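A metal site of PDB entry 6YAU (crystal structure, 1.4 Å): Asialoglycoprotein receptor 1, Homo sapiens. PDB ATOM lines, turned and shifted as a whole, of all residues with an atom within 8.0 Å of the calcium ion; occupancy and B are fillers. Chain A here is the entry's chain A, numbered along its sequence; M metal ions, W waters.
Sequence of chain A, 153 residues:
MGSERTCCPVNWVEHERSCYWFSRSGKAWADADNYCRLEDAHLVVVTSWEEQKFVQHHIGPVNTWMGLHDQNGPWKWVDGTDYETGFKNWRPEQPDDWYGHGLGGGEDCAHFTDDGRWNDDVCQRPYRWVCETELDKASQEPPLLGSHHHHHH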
ATOM      1  N   HIS A  15      21.176  27.350  28.591  1.00  0.00           N
ATOM      2  CA  HIS A  15      22.235  28.004  27.841  1.00  0.00           C
ATOM      3  C   HIS A  15      21.944  27.908  26.382  1.00  0.00           C
ATOM      4  O   HIS A  15      21.852  26.801  25.833  1.00  0.00           O
ATOM      5  CB  HIS A  15      23.632  27.427  28.131  1.00  0.00           C
ATOM      6  CG  HIS A  15      24.744  28.077  27.345  1.00  0.00           C
ATOM      7  ND1 HIS A  15      25.239  29.322  27.694  1.00  0.00           N
ATOM      8  CD2 HIS A  15      25.413  27.626  26.257  1.00  0.00           C
ATOM      9  CE1 HIS A  15      26.188  29.592  26.805  1.00  0.00           C
ATOM     10  NE2 HIS A  15      26.333  28.600  25.927  1.00  0.00           N
ATOM     11  N   GLU A  16      21.753  29.070  25.705  1.00  0.00           N
ATOM     12  CA  GLU A  16      21.471  29.139  24.259  1.00  0.00           C
ATOM     13  C   GLU A  16      20.470  28.091  23.759  1.00  0.00           C
ATOM     14  O   GLU A  16      20.820  27.262  22.903  1.00  0.00           O
ATOM     15  CB  GLU A  16      22.727  28.940  23.411  1.00  0.00           C
ATOM     16  CG  GLU A  16      23.891  29.923  23.520  1.00  0.00           C
ATOM     17  CD  GLU A  16      23.631  31.320  22.963  1.00  0.00           C
ATOM     18  OE1 GLU A  16      23.194  31.426  21.805  1.00  0.00           O
ATOM     19  OE2 GLU A  16      23.884  32.299  23.702  1.00  0.00           O
ATOM     20  N   SER A  18      19.314  25.376  25.014  1.00  0.00           N
ATOM     21  CA  SER A  18      19.490  24.000  25.503  1.00  0.00           C
ATOM     22  C   SER A  18      19.449  24.011  27.032  1.00  0.00           C
ATOM     23  O   SER A  18      19.799  25.010  27.661  1.00  0.00           O
ATOM     24  CB  SER A  18      20.812  23.410  25.009  1.00  0.00           C
ATOM     25  OG  SER A  18      20.716  22.801  23.737  1.00  0.00           O
ATOM     26  N   CYS A  19      19.031  22.883  27.616  1.00  0.00           N
ATOM     27  CA  CYS A  19      18.986  22.616  29.055  1.00  0.00           C
ATOM     28  C   CYS A  19      20.049  21.574  29.318  1.00  0.00           C
ATOM     29  O   CYS A  19      20.081  20.573  28.618  1.00  0.00           O
ATOM     30  CB  CYS A  19      17.616  22.087  29.468  1.00  0.00           C
ATOM     31  SG  CYS A  19      16.259  23.182  29.026  1.00  0.00           S
ATOM     32  N   TYR A  20      20.820  21.762  30.380  1.00  0.00           N
ATOM     33  CA  TYR A  20      21.894  20.839  30.744  1.00  0.00           C
ATOM     34  C   TYR A  20      21.801  20.396  32.165  1.00  0.00           C
ATOM     35  O   TYR A  20      21.484  21.198  33.053  1.00  0.00           O
ATOM     36  CB  TYR A  20      23.294  21.488  30.533  1.00  0.00           C
ATOM     37  CG  TYR A  20      23.533  22.014  29.143  1.00  0.00           C
ATOM     38  CD1 TYR A  20      23.012  23.239  28.737  1.00  0.00           C
ATOM     39  CD2 TYR A  20      24.320  21.306  28.240  1.00  0.00           C
ATOM     40  CE1 TYR A  20      23.265  23.750  27.469  1.00  0.00           C
ATOM     41  CE2 TYR A  20      24.570  21.804  26.960  1.00  0.00           C
ATOM     42  CZ  TYR A  20      24.030  23.018  26.573  1.00  0.00           C
ATOM     43  OH  TYR A  20      24.271  23.522  25.332  1.00  0.00           O
ATOM     44  N   HIS A  42      19.727  13.559  26.128  1.00  0.00           N
ATOM     45  CA  HIS A  42      20.812  12.800  25.526  1.00  0.00           C
ATOM     46  C   HIS A  42      22.112  13.258  26.118  1.00  0.00           C
ATOM     47  O   HIS A  42      22.185  14.389  26.626  1.00  0.00           O
ATOM     48  CB  HIS A  42      20.840  12.977  23.999  1.00  0.00           C
ATOM     49  CG  HIS A  42      20.948  14.411  23.554  1.00  0.00           C
ATOM     50  ND1 HIS A  42      22.173  15.050  23.475  1.00  0.00           N
ATOM     51  CD2 HIS A  42      19.977  15.265  23.156  1.00  0.00           C
ATOM     52  CE1 HIS A  42      21.911  16.274  23.047  1.00  0.00           C
ATOM     53  NE2 HIS A  42      20.601  16.451  22.839  1.00  0.00           N
ATOM     54  N   LEU A  43      23.148  12.387  26.058  1.00  0.00           N
ATOM     55  CA  LEU A  43      24.472  12.791  26.538  1.00  0.00           C
ATOM     56  C   LEU A  43      24.883  14.031  25.719  1.00  0.00           C
ATOM     57  O   LEU A  43      24.557  14.108  24.550  1.00  0.00           O
ATOM     58  CB  LEU A  43      25.483  11.652  26.416  1.00  0.00           C
ATOM     59  CG  LEU A  43      25.504  10.631  27.559  1.00  0.00           C
ATOM     60  CD1 LEU A  43      26.303   9.409  27.147  1.00  0.00           C
ATOM     61  CD2 LEU A  43      26.104  11.262  28.865  1.00  0.00           C
ATOM     62  N   VAL A  44      25.475  15.030  26.363  1.00  0.00           N
ATOM     63  CA  VAL A  44      25.744  16.327  25.744  1.00  0.00           C
ATOM     64  C   VAL A  44      26.426  16.207  24.387  1.00  0.00           C
ATOM     65  O   VAL A  44      27.394  15.459  24.227  1.00  0.00           O
ATOM     66  CB  VAL A  44      26.520  17.290  26.698  1.00  0.00           C
ATOM     67  CG1 VAL A  44      27.964  16.797  26.979  1.00  0.00           C
ATOM     68  CG2 VAL A  44      26.511  18.726  26.170  1.00  0.00           C
ATOM     69  N   VAL A  45      25.918  16.984  23.409  1.00  0.00           N
ATOM     70  CA  VAL A  45      26.464  17.018  22.058  1.00  0.00           C
ATOM     71  C   VAL A  45      27.071  18.423  21.885  1.00  0.00           C
ATOM     72  O   VAL A  45      26.356  19.408  21.927  1.00  0.00           O
ATOM     73  CB  VAL A  45      25.370  16.703  21.003  1.00  0.00           C
ATOM     74  CG1 VAL A  45      25.865  17.030  19.586  1.00  0.00           C
ATOM     75  CG2 VAL A  45      24.906  15.254  21.087  1.00  0.00           C
ATOM     76  N   VAL A  46      28.398  18.511  21.739  1.00  0.00           N
ATOM     77  CA  VAL A  46      29.093  19.792  21.689  1.00  0.00           C
ATOM     78  C   VAL A  46      29.356  20.206  20.243  1.00  0.00           C
ATOM     79  O   VAL A  46      30.125  19.533  19.573  1.00  0.00           O
ATOM     80  CB  VAL A  46      30.411  19.730  22.509  1.00  0.00           C
ATOM     81  CG1 VAL A  46      31.158  21.075  22.489  1.00  0.00           C
ATOM     82  CG2 VAL A  46      30.124  19.279  23.940  1.00  0.00           C
ATOM     83  N   THR A  47      28.755  21.340  19.793  1.00  0.00           N
ATOM     84  CA  THR A  47      28.878  21.766  18.393  1.00  0.00           C
ATOM     85  C   THR A  47      29.487  23.161  18.160  1.00  0.00           C
ATOM     86  O   THR A  47      29.484  23.640  17.023  1.00  0.00           O
ATOM     87  CB  THR A  47      27.511  21.673  17.708  1.00  0.00           C
ATOM     88  OG1 THR A  47      26.581  22.496  18.432  1.00  0.00           O
ATOM     89  CG2 THR A  47      27.008  20.227  17.567  1.00  0.00           C
ATOM     90  N   SER A  48      30.044  23.792  19.209  1.00  0.00           N
ATOM     91  CA  SER A  48      30.705  25.089  19.085  1.00  0.00           C
ATOM     92  C   SER A  48      31.684  25.303  20.212  1.00  0.00           C
ATOM     93  O   SER A  48      31.575  24.657  21.255  1.00  0.00           O
ATOM     94  CB  SER A  48      29.681  26.220  19.084  1.00  0.00           C
ATOM     95  OG  SER A  48      29.057  26.362  20.358  1.00  0.00           O
ATOM     96  N   GLU A  51      29.702  26.521  23.370  1.00  0.00           N
ATOM     97  CA  GLU A  51      29.106  25.417  24.129  1.00  0.00           C
ATOM     98  C   GLU A  51      30.194  24.649  24.908  1.00  0.00           C
ATOM     99  O   GLU A  51      30.006  24.372  26.088  1.00  0.00           O
ATOM    100  CB  GLU A  51      28.315  24.491  23.216  1.00  0.00           C
ATOM    101  CG  GLU A  51      27.517  23.456  23.978  1.00  0.00           C
ATOM    102  CD  GLU A  51      26.623  22.598  23.110  1.00  0.00           C
ATOM    103  OE1 GLU A  51      25.720  21.943  23.675  1.00  0.00           O
ATOM    104  OE2 GLU A  51      26.826  22.574  21.880  1.00  0.00           O
ATOM    105  N   VAL A  55      30.181  24.219  28.929  1.00  0.00           N
ATOM    106  CA  VAL A  55      30.239  22.924  29.603  1.00  0.00           C
ATOM    107  C   VAL A  55      31.466  22.855  30.524  1.00  0.00           C
ATOM    108  O   VAL A  55      31.324  22.443  31.680  1.00  0.00           O
ATOM    109  CB  VAL A  55      30.187  21.740  28.599  1.00  0.00           C
ATOM    110  CG1 VAL A  55      30.331  20.401  29.330  1.00  0.00           C
ATOM    111  CG2 VAL A  55      28.880  21.774  27.808  1.00  0.00           C
ATOM    112  N   TRP A  77      27.857  11.328  16.960  1.00  0.00           N
ATOM    113  CA  TRP A  77      27.170  12.033  18.064  1.00  0.00           C
ATOM    114  C   TRP A  77      25.860  11.275  18.317  1.00  0.00           C
ATOM    115  O   TRP A  77      25.230  10.809  17.372  1.00  0.00           O
ATOM    116  CB  TRP A  77      26.898  13.503  17.702  1.00  0.00           C
ATOM    117  CG  TRP A  77      28.154  14.321  17.669  1.00  0.00           C
ATOM    118  CD1 TRP A  77      28.830  14.737  16.569  1.00  0.00           C
ATOM    119  CD2 TRP A  77      28.869  14.833  18.808  1.00  0.00           C
ATOM    120  NE1 TRP A  77      29.943  15.459  16.938  1.00  0.00           N
ATOM    121  CE2 TRP A  77      29.973  15.568  18.309  1.00  0.00           C
ATOM    122  CE3 TRP A  77      28.676  14.759  20.193  1.00  0.00           C
ATOM    123  CZ2 TRP A  77      30.882  16.205  19.144  1.00  0.00           C
ATOM    124  CZ3 TRP A  77      29.580  15.404  21.028  1.00  0.00           C
ATOM    125  CH2 TRP A  77      30.670  16.108  20.506  1.00  0.00           C
ATOM    126  N   ASP A  79      22.871  12.123  18.995  1.00  0.00           N
ATOM    127  CA  ASP A  79      21.606  12.617  18.431  1.00  0.00           C
ATOM    128  C   ASP A  79      21.595  12.703  16.884  1.00  0.00           C
ATOM    129  O   ASP A  79      20.694  13.334  16.317  1.00  0.00           O
ATOM    130  CB  ASP A  79      21.221  13.969  19.077  1.00  0.00           C
ATOM    131  CG  ASP A  79      22.135  15.112  18.688  1.00  0.00           C
ATOM    132  OD1 ASP A  79      23.174  14.857  18.034  1.00  0.00           O
ATOM    133  OD2 ASP A  79      21.821  16.266  19.055  1.00  0.00           O
ATOM    134  N   THR A  81      23.898  14.234  14.985  1.00  0.00           N
ATOM    135  CA  THR A  81      24.738  15.348  14.504  1.00  0.00           C
ATOM    136  C   THR A  81      25.990  14.788  13.813  1.00  0.00           C
ATOM    137  O   THR A  81      26.616  13.875  14.351  1.00  0.00           O
ATOM    138  CB  THR A  81      25.127  16.285  15.668  1.00  0.00           C
ATOM    139  OG1 THR A  81      23.954  16.659  16.385  1.00  0.00           O
ATOM    140  CG2 THR A  81      25.850  17.539  15.205  1.00  0.00           C
ATOM    141  N   GLU A 132      21.783  16.691  28.071  1.00  0.00           N
ATOM    142  CA  GLU A 132      21.335  17.868  27.348  1.00  0.00           C
ATOM    143  C   GLU A 132      19.999  17.597  26.674  1.00  0.00           C
ATOM    144  O   GLU A 132      19.779  16.510  26.133  1.00  0.00           O
ATOM    145  CB  GLU A 132      22.385  18.267  26.297  1.00  0.00           C
ATOM    146  CG  GLU A 132      22.006  19.507  25.494  1.00  0.00           C
ATOM    147  CD  GLU A 132      22.918  19.850  24.334  1.00  0.00           C
ATOM    148  OE1 GLU A 132      23.791  19.038  23.968  1.00  0.00           O
ATOM    149  OE2 GLU A 132      22.747  20.965  23.787  1.00  0.00           O
ATOM    150  N   THR A 133      19.138  18.626  26.672  1.00  0.00           N
ATOM    151  CA  THR A 133      17.875  18.604  25.953  1.00  0.00           C
ATOM    152  C   THR A 133      17.741  19.960  25.245  1.00  0.00           C
ATOM    153  O   THR A 133      18.289  20.958  25.713  1.00  0.00           O
ATOM    154  CB  THR A 133      16.708  18.163  26.857  1.00  0.00           C
ATOM    155  OG1 THR A 133      15.630  17.741  26.029  1.00  0.00           O
ATOM    156  CG2 THR A 133      16.233  19.232  27.797  1.00  0.00           C
ATOM    157  N   GLU A 134      17.112  19.979  24.070  1.00  0.00           N
ATOM    158  CA  GLU A 134      16.934  21.219  23.320  1.00  0.00           C
ATOM    159  C   GLU A 134      15.552  21.754  23.572  1.00  0.00           C
ATOM    160  O   GLU A 134      14.583  20.996  23.549  1.00  0.00           O
ATOM    161  CB  GLU A 134      17.134  21.011  21.795  1.00  0.00           C
ATOM    162  CG  GLU A 134      18.575  20.717  21.393  1.00  0.00           C
ATOM    163  CD  GLU A 134      19.037  19.298  21.688  1.00  0.00           C
ATOM    164  OE1 GLU A 134      20.203  19.129  22.133  1.00  0.00           O
ATOM    165  OE2 GLU A 134      18.244  18.354  21.500  1.00  0.00           O
HETATM  166 CA    CA M   1      24.464  20.896  22.120  1.00  0.00          CA
HETATM  167  O   HOH W   1      23.371  23.120  21.591  1.00  0.00           O
HETATM  168  O   HOH W   2      22.660  19.511  21.038  1.00  0.00           O
HETATM  169  O   HOH W   3      24.734  20.999  19.767  1.00  0.00           O
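Water W3 bridges the side-chain hydroxyl of Thr 47 (2.7 Å) and the side-chain carboxylate of Glu 51 (3.4 Å).
OE1 of Glu 51 sits close to OH of Tyr 20 (2.7 Å). OE2 of Glu 132 sits close to OG of Ser 18 (2.7 Å). The side-chain carboxylate (OE2) of Glu 132 sits close to the side-chain hydroxyl (OH) of Tyr 20, 3.4 Å away. The side-chain carboxylate of Glu 51 is in hydrogen-bond range of the backbone NH of Thr 47. The backbone NH (N) of Glu 132 is in hydrogen-bond range of the backbone carbonyl oxygen (O) of His 42 (2.7 Å). N of Glu 51 is in hydrogen-bond range of OG of Ser 48.
Along chain A the residues within 4 Å of the calcium ion span positions 45 to 132. The nearest printed residue that does not touch the calcium ion is Tyr 20 (4.2 Å).
The calcium ion is bound by OE1 of Glu 51 (2.3 Å), water W3 (2.4 Å), OE2 of Glu 132 (2.4 Å), O of Val 45 (2.4 Å), water W2 (2.5 Å), water W1 (2.5 Å) and OE1 of Glu 132 (2.7 Å). The calcium ion has seven donor atoms within binding distance. Slightly farther from the calcium ion lies OE2 of Glu 51 (2.9 Å).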
